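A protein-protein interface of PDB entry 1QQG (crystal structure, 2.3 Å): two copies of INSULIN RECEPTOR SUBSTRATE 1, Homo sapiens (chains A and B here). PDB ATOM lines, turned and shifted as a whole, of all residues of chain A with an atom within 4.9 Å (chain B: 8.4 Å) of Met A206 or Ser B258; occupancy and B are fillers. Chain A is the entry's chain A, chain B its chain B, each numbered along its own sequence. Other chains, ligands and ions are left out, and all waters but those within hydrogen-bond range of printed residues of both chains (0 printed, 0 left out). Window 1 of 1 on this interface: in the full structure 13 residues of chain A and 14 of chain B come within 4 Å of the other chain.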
ATOM      1  N   GLN A 204     -15.018 -19.804  36.842  1.00  0.00           N
ATOM      2  CA  GLN A 204     -13.793 -19.727  36.031  1.00  0.00           C
ATOM      3  C   GLN A 204     -13.507 -18.230  35.960  1.00  0.00           C
ATOM      4  O   GLN A 204     -14.441 -17.444  35.783  1.00  0.00           O
ATOM      5  CB  GLN A 204     -14.044 -20.252  34.609  1.00  0.00           C
ATOM      6  CG  GLN A 204     -14.679 -21.635  34.529  1.00  0.00           C
ATOM      7  CD  GLN A 204     -13.745 -22.726  35.008  1.00  0.00           C
ATOM      8  OE1 GLN A 204     -12.558 -22.751  34.636  1.00  0.00           O
ATOM      9  NE2 GLN A 204     -14.259 -23.628  35.854  1.00  0.00           N
ATOM     10  N   LEU A 205     -12.249 -17.829  36.131  1.00  0.00           N
ATOM     11  CA  LEU A 205     -11.897 -16.408  36.074  1.00  0.00           C
ATOM     12  C   LEU A 205     -12.370 -15.719  34.779  1.00  0.00           C
ATOM     13  O   LEU A 205     -12.859 -14.590  34.811  1.00  0.00           O
ATOM     14  CB  LEU A 205     -10.387 -16.213  36.270  1.00  0.00           C
ATOM     15  CG  LEU A 205      -9.859 -16.481  37.689  1.00  0.00           C
ATOM     16  CD1 LEU A 205      -8.370 -16.146  37.800  1.00  0.00           C
ATOM     17  CD2 LEU A 205     -10.666 -15.672  38.699  1.00  0.00           C
ATOM     18  N   MET A 206     -12.297 -16.434  33.660  1.00  0.00           N
ATOM     19  CA  MET A 206     -12.715 -15.912  32.365  1.00  0.00           C
ATOM     20  C   MET A 206     -14.182 -15.497  32.315  1.00  0.00           C
ATOM     21  O   MET A 206     -14.578 -14.687  31.471  1.00  0.00           O
ATOM     22  CB  MET A 206     -12.437 -16.941  31.269  1.00  0.00           C
ATOM     23  CG  MET A 206     -10.966 -17.260  31.090  1.00  0.00           C
ATOM     24  SD  MET A 206     -10.655 -18.564  29.887  1.00  0.00           S
ATOM     25  CE  MET A 206     -12.296 -19.430  29.809  1.00  0.00           C
ATOM     26  N   ASN A 207     -14.980 -16.057  33.215  1.00  0.00           N
ATOM     27  CA  ASN A 207     -16.407 -15.763  33.289  1.00  0.00           C
ATOM     28  C   ASN A 207     -16.742 -14.484  34.048  1.00  0.00           C
ATOM     29  O   ASN A 207     -17.854 -13.991  33.953  1.00  0.00           O
ATOM     30  CB  ASN A 207     -17.150 -16.938  33.920  1.00  0.00           C
ATOM     31  CG  ASN A 207     -17.066 -18.193  33.080  1.00  0.00           C
ATOM     32  OD1 ASN A 207     -16.279 -18.280  32.133  1.00  0.00           O
ATOM     33  ND2 ASN A 207     -17.897 -19.168  33.406  1.00  0.00           N
ATOM     34  N   ILE A 208     -15.793 -13.942  34.802  1.00  0.00           N
ATOM     35  CA  ILE A 208     -16.070 -12.716  35.548  1.00  0.00           C
ATOM     36  C   ILE A 208     -16.034 -11.499  34.633  1.00  0.00           C
ATOM     37  O   ILE A 208     -15.077 -11.310  33.892  1.00  0.00           O
ATOM     38  CB  ILE A 208     -15.060 -12.494  36.713  1.00  0.00           C
ATOM     39  CG1 ILE A 208     -15.006 -13.742  37.602  1.00  0.00           C
ATOM     40  CG2 ILE A 208     -15.461 -11.272  37.539  1.00  0.00           C
ATOM     41  CD1 ILE A 208     -13.998 -13.666  38.724  1.00  0.00           C
ATOM     42  N   ARG A 209     -17.101 -10.711  34.633  1.00  0.00           N
ATOM     43  CA  ARG A 209     -17.122  -9.499  33.828  1.00  0.00           C
ATOM     44  C   ARG A 209     -16.376  -8.392  34.573  1.00  0.00           C
ATOM     45  O   ARG A 209     -15.514  -7.727  34.007  1.00  0.00           O
ATOM     46  CB  ARG A 209     -18.555  -9.068  33.503  1.00  0.00           C
ATOM     47  CG  ARG A 209     -19.163  -9.824  32.337  1.00  0.00           C
ATOM     48  CD  ARG A 209     -20.497  -9.246  31.919  1.00  0.00           C
ATOM     49  NE  ARG A 209     -20.439  -7.788  31.849  1.00  0.00           N
ATOM     50  CZ  ARG A 209     -20.503  -7.072  30.730  1.00  0.00           C
ATOM     51  NH1 ARG A 209     -20.626  -7.657  29.545  1.00  0.00           N
ATOM     52  NH2 ARG A 209     -20.455  -5.752  30.814  1.00  0.00           N
ATOM     53  N   GLY A 223     -20.384 -13.346  33.951  1.00  0.00           N
ATOM     54  CA  GLY A 223     -21.050 -13.232  32.661  1.00  0.00           C
ATOM     55  C   GLY A 223     -22.007 -14.370  32.364  1.00  0.00           C
ATOM     56  O   GLY A 223     -22.217 -15.245  33.212  1.00  0.00           O
ATOM     57  N   ARG A 224     -22.571 -14.376  31.155  1.00  0.00           N
ATOM     58  CA  ARG A 224     -23.518 -15.418  30.756  1.00  0.00           C
ATOM     59  C   ARG A 224     -22.899 -16.809  30.741  1.00  0.00           C
ATOM     60  O   ARG A 224     -23.573 -17.788  31.058  1.00  0.00           O
ATOM     61  CB  ARG A 224     -24.135 -15.135  29.378  1.00  0.00           C
ATOM     62  CG  ARG A 224     -25.035 -13.907  29.294  1.00  0.00           C
ATOM     63  CD  ARG A 224     -25.806 -13.900  27.973  1.00  0.00           C
ATOM     64  NE  ARG A 224     -24.941 -14.197  26.829  1.00  0.00           N
ATOM     65  CZ  ARG A 224     -25.362 -14.435  25.588  1.00  0.00           C
ATOM     66  NH1 ARG A 224     -26.655 -14.412  25.286  1.00  0.00           N
ATOM     67  NH2 ARG A 224     -24.475 -14.718  24.641  1.00  0.00           N
ATOM     68  N   SER A 225     -21.623 -16.900  30.381  1.00  0.00           N
ATOM     69  CA  SER A 225     -20.947 -18.193  30.332  1.00  0.00           C
ATOM     70  C   SER A 225     -20.747 -18.806  31.719  1.00  0.00           C
ATOM     71  O   SER A 225     -20.271 -19.929  31.848  1.00  0.00           O
ATOM     72  CB  SER A 225     -19.609 -18.071  29.616  1.00  0.00           C
ATOM     73  OG  SER A 225     -18.718 -17.305  30.391  1.00  0.00           O
ATOM     74  N   ALA A 226     -21.115 -18.062  32.757  1.00  0.00           N
ATOM     75  CA  ALA A 226     -20.986 -18.550  34.125  1.00  0.00           C
ATOM     76  C   ALA A 226     -21.920 -19.724  34.379  1.00  0.00           C
ATOM     77  O   ALA A 226     -23.053 -19.757  33.893  1.00  0.00           O
ATOM     78  CB  ALA A 226     -21.269 -17.428  35.130  1.00  0.00           C
ATOM     79  N   MET A 257      -4.129 -13.464  33.289  1.00  0.00           N
ATOM     80  CA  MET A 257      -4.487 -14.539  32.388  1.00  0.00           C
ATOM     81  C   MET A 257      -4.113 -14.235  30.952  1.00  0.00           C
ATOM     82  O   MET A 257      -3.910 -15.152  30.158  1.00  0.00           O
ATOM     83  CB  MET A 257      -5.962 -14.875  32.490  1.00  0.00           C
ATOM     84  CG  MET A 257      -6.308 -15.707  33.707  1.00  0.00           C
ATOM     85  SD  MET A 257      -7.787 -16.638  33.354  1.00  0.00           S
ATOM     86  CE  MET A 257      -8.950 -15.241  33.012  1.00  0.00           C
ATOM     87  N   MET B 206      -8.488 -10.728  24.010  1.00  0.00           N
ATOM     88  CA  MET B 206      -8.028 -11.640  25.062  1.00  0.00           C
ATOM     89  C   MET B 206      -6.674 -11.267  25.627  1.00  0.00           C
ATOM     90  O   MET B 206      -6.358 -11.614  26.756  1.00  0.00           O
ATOM     91  CB  MET B 206      -7.862 -13.059  24.535  1.00  0.00           C
ATOM     92  CG  MET B 206      -9.118 -13.841  24.283  1.00  0.00           C
ATOM     93  SD  MET B 206      -8.709 -15.573  23.951  1.00  0.00           S
ATOM     94  CE  MET B 206      -7.148 -15.414  22.959  1.00  0.00           C
ATOM     95  N   GLU B 252     -15.857  -2.522  27.828  1.00  0.00           N
ATOM     96  CA  GLU B 252     -17.119  -3.249  27.712  1.00  0.00           C
ATOM     97  C   GLU B 252     -17.006  -4.394  26.720  1.00  0.00           C
ATOM     98  O   GLU B 252     -17.645  -5.430  26.873  1.00  0.00           O
ATOM     99  CB  GLU B 252     -18.232  -2.312  27.271  1.00  0.00           C
ATOM    100  CG  GLU B 252     -19.541  -3.020  26.956  1.00  0.00           C
ATOM    101  CD  GLU B 252     -19.989  -3.954  28.069  1.00  0.00           C
ATOM    102  OE1 GLU B 252     -20.511  -5.051  27.759  1.00  0.00           O
ATOM    103  OE2 GLU B 252     -19.821  -3.593  29.250  1.00  0.00           O
ATOM    104  N   ALA B 253     -16.195  -4.197  25.687  1.00  0.00           N
ATOM    105  CA  ALA B 253     -16.009  -5.232  24.693  1.00  0.00           C
ATOM    106  C   ALA B 253     -15.164  -6.330  25.302  1.00  0.00           C
ATOM    107  O   ALA B 253     -15.275  -7.486  24.911  1.00  0.00           O
ATOM    108  CB  ALA B 253     -15.345  -4.660  23.456  1.00  0.00           C
ATOM    109  N   MET B 254     -14.308  -5.954  26.251  1.00  0.00           N
ATOM    110  CA  MET B 254     -13.430  -6.904  26.938  1.00  0.00           C
ATOM    111  C   MET B 254     -14.264  -7.756  27.885  1.00  0.00           C
ATOM    112  O   MET B 254     -14.172  -8.990  27.892  1.00  0.00           O
ATOM    113  CB  MET B 254     -12.343  -6.164  27.716  1.00  0.00           C
ATOM    114  CG  MET B 254     -11.071  -5.900  26.922  1.00  0.00           C
ATOM    115  SD  MET B 254     -10.078  -4.541  27.613  1.00  0.00           S
ATOM    116  CE  MET B 254      -9.289  -5.290  29.063  1.00  0.00           C
ATOM    117  N   ARG B 255     -15.130  -7.085  28.629  1.00  0.00           N
ATOM    118  CA  ARG B 255     -15.998  -7.747  29.582  1.00  0.00           C
ATOM    119  C   ARG B 255     -17.039  -8.613  28.895  1.00  0.00           C
ATOM    120  O   ARG B 255     -17.349  -9.698  29.368  1.00  0.00           O
ATOM    121  CB  ARG B 255     -16.661  -6.696  30.454  1.00  0.00           C
ATOM    122  CG  ARG B 255     -15.638  -5.865  31.208  1.00  0.00           C
ATOM    123  CD  ARG B 255     -16.268  -4.736  31.995  1.00  0.00           C
ATOM    124  NE  ARG B 255     -15.377  -4.295  33.057  1.00  0.00           N
ATOM    125  CZ  ARG B 255     -15.612  -3.254  33.844  1.00  0.00           C
ATOM    126  NH1 ARG B 255     -16.706  -2.518  33.682  1.00  0.00           N
ATOM    127  NH2 ARG B 255     -14.786  -2.997  34.850  1.00  0.00           N
ATOM    128  N   ALA B 256     -17.527  -8.162  27.744  1.00  0.00           N
ATOM    129  CA  ALA B 256     -18.541  -8.888  26.984  1.00  0.00           C
ATOM    130  C   ALA B 256     -18.082 -10.268  26.510  1.00  0.00           C
ATOM    131  O   ALA B 256     -18.888 -11.079  26.048  1.00  0.00           O
ATOM    132  CB  ALA B 256     -18.999  -8.047  25.798  1.00  0.00           C
ATOM    133  N   MET B 257     -16.785 -10.528  26.617  1.00  0.00           N
ATOM    134  CA  MET B 257     -16.218 -11.801  26.196  1.00  0.00           C
ATOM    135  C   MET B 257     -16.695 -12.951  27.087  1.00  0.00           C
ATOM    136  O   MET B 257     -16.808 -14.102  26.641  1.00  0.00           O
ATOM    137  CB  MET B 257     -14.701 -11.714  26.248  1.00  0.00           C
ATOM    138  CG  MET B 257     -14.127 -10.667  25.335  1.00  0.00           C
ATOM    139  SD  MET B 257     -13.614 -11.397  23.798  1.00  0.00           S
ATOM    140  CE  MET B 257     -11.871 -11.647  24.184  1.00  0.00           C
ATOM    141  N   SER B 258     -16.955 -12.638  28.356  1.00  0.00           N
ATOM    142  CA  SER B 258     -17.417 -13.638  29.309  1.00  0.00           C
ATOM    143  C   SER B 258     -18.887 -13.965  29.084  1.00  0.00           C
ATOM    144  O   SER B 258     -19.446 -14.837  29.748  1.00  0.00           O
ATOM    145  CB  SER B 258     -17.161 -13.178  30.749  1.00  0.00           C
ATOM    146  OG  SER B 258     -17.790 -11.949  31.028  1.00  0.00           O
ATOM    147  N   ASP B 259     -19.499 -13.265  28.131  1.00  0.00           N
ATOM    148  CA  ASP B 259     -20.895 -13.489  27.778  1.00  0.00           C
ATOM    149  C   ASP B 259     -21.042 -14.425  26.587  1.00  0.00           C
ATOM    150  O   ASP B 259     -22.151 -14.810  26.235  1.00  0.00           O
ATOM    151  CB  ASP B 259     -21.595 -12.170  27.488  1.00  0.00           C
ATOM    152  CG  ASP B 259     -21.705 -11.302  28.706  1.00  0.00           C
ATOM    153  OD1 ASP B 259     -21.970 -11.839  29.799  1.00  0.00           O
ATOM    154  OD2 ASP B 259     -21.536 -10.077  28.577  1.00  0.00           O
ATOM    155  N   GLU B 260     -19.924 -14.781  25.962  1.00  0.00           N
ATOM    156  CA  GLU B 260     -19.966 -15.685  24.819  1.00  0.00           C
ATOM    157  C   GLU B 260     -19.865 -17.131  25.314  1.00  0.00           C
ATOM    158  O   GLU B 260     -19.034 -17.447  26.168  1.00  0.00           O
ATOM    159  CB  GLU B 260     -18.829 -15.373  23.833  1.00  0.00           C
ATOM    160  CG  GLU B 260     -18.534 -13.865  23.625  1.00  0.00           C
ATOM    161  CD  GLU B 260     -19.553 -13.088  22.753  1.00  0.00           C
ATOM    162  OE1 GLU B 260     -19.165 -12.005  22.240  1.00  0.00           O
ATOM    163  OE2 GLU B 260     -20.719 -13.535  22.588  1.00  0.00           O
ATOM    164  N   PHE B 261     -20.744 -17.999  24.823  1.00  0.00           N
ATOM    165  CA  PHE B 261     -20.714 -19.398  25.226  1.00  0.00           C
ATOM    166  C   PHE B 261     -19.606 -20.125  24.450  1.00  0.00           C
ATOM    167  O   PHE B 261     -19.769 -20.330  23.231  1.00  0.00           O
ATOM    168  CB  PHE B 261     -22.067 -20.065  24.963  1.00  0.00           C
ATOM    169  CG  PHE B 261     -23.218 -19.420  25.675  1.00  0.00           C
ATOM    170  CD1 PHE B 261     -24.265 -18.858  24.954  1.00  0.00           C
ATOM    171  CD2 PHE B 261     -23.257 -19.378  27.067  1.00  0.00           C
ATOM    172  CE1 PHE B 261     -25.343 -18.264  25.604  1.00  0.00           C
ATOM    173  CE2 PHE B 261     -24.327 -18.786  27.737  1.00  0.00           C
ATOM    174  CZ  PHE B 261     -25.377 -18.224  27.002  1.00  0.00           C
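The guanidinium group of Arg A209 lies within salt-bridge range of the side-chain carboxylate of Asp B259.
The guanidinium group of Arg A224 sits at hydrogen-bond distance from the backbone carbonyl oxygen of Asp B259, at 2.8 Å.
NH2 of Arg A209 is in salt-bridge range of OE2 of Glu B252, 2.7 Å away.
The backbone carbonyl oxygen (O) of Ser B258 sits at hydrogen-bond distance from the backbone NH (N) of Arg A224 (3.5 Å).
OG of Ser A225 is in hydrogen-bond range of O of Ser B258, 2.7 Å away.
The side-chain amide nitrogen of Asn A207 lies close to the backbone NH of Ala A226 (3.5 Å).
The backbone carbonyl oxygen of Arg B255 lies within hydrogen-bond range of the side-chain hydroxyl of Ser B258.
ND2 of Asn A207 lies within hydrogen-bond range of O of Ser A225 (2.9 Å).
The backbone carbonyl oxygen (O) of Asn A207 lies within hydrogen-bond range of the backbone NH (N) of Gly A223 (2.6 Å).
Met A206 touches Ser B258.
O of Asn A207 touches CB of Ser B258 (3.4 Å).
Ser B258 touches Ile A208 (OG to O, 3.996 Å).
Arg B255 touches Arg A209.
NH1 of Arg A209 touches CA of Ala B256, at 3.5 Å.
Arg A209 touches Ser B258 (CG to OG, 2.8 Å).
Gly A223 touches Ser B258 (C to O, 3.7 Å).
Gly A223 touches Asp B259.
Arg A224 touches Phe B261.
Glu B260 touches Ser A225 (O to CB, 3.6 Å).
Hydrophobic or aromatic side chains of chain B that line the printed part of chain A: Phe B261.
Of the 11 printed residues of chain A, 7 touch a printed residue of chain B.
Among the printed residues, Asp or Glu carboxylates within 4 Å of a Lys or Arg side-chain nitrogen of the other chain: Arg A209 with Glu B252 (2.7 Å) and Arg A209 with Asp B259 (2.8 Å).
Positions printed for both chains: 206 and 257.
Of the 15 pairs that touch across the chains among the printed residues, none has its exchanged pair printed and touching as well.
Gln A204 touches none of the printed residues of chain B.
Met A206 touches one residue of chain B.
Of the printed residues of chain B, Asn A207 touches Ser B258 (3.4 Å).
Of the printed residues of chain B, Ile A208 touches Ser B258.
Printed residues of chain B within 4 Å of Ser A225: Ser B258 and Glu B260.
Printed residues of chain A within 4 Å of Glu B252: Arg A209 (2.7 Å).
Of the printed residues of chain A, Ser B258 touches Met A206, Asn A207, Ile A208, Arg A209, Gly A223, Arg A224 and Ser A225.
Of the printed residues of chain A, Asp B259 touches Arg A209, Gly A223 and Arg A224.
The nearest printed residue of chain A that does not touch Ser B258 is Ala A226 (4.7 Å).
The nearest printed residue of chain A that does not touch Arg B255 is Ile A208 (5.3 Å).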
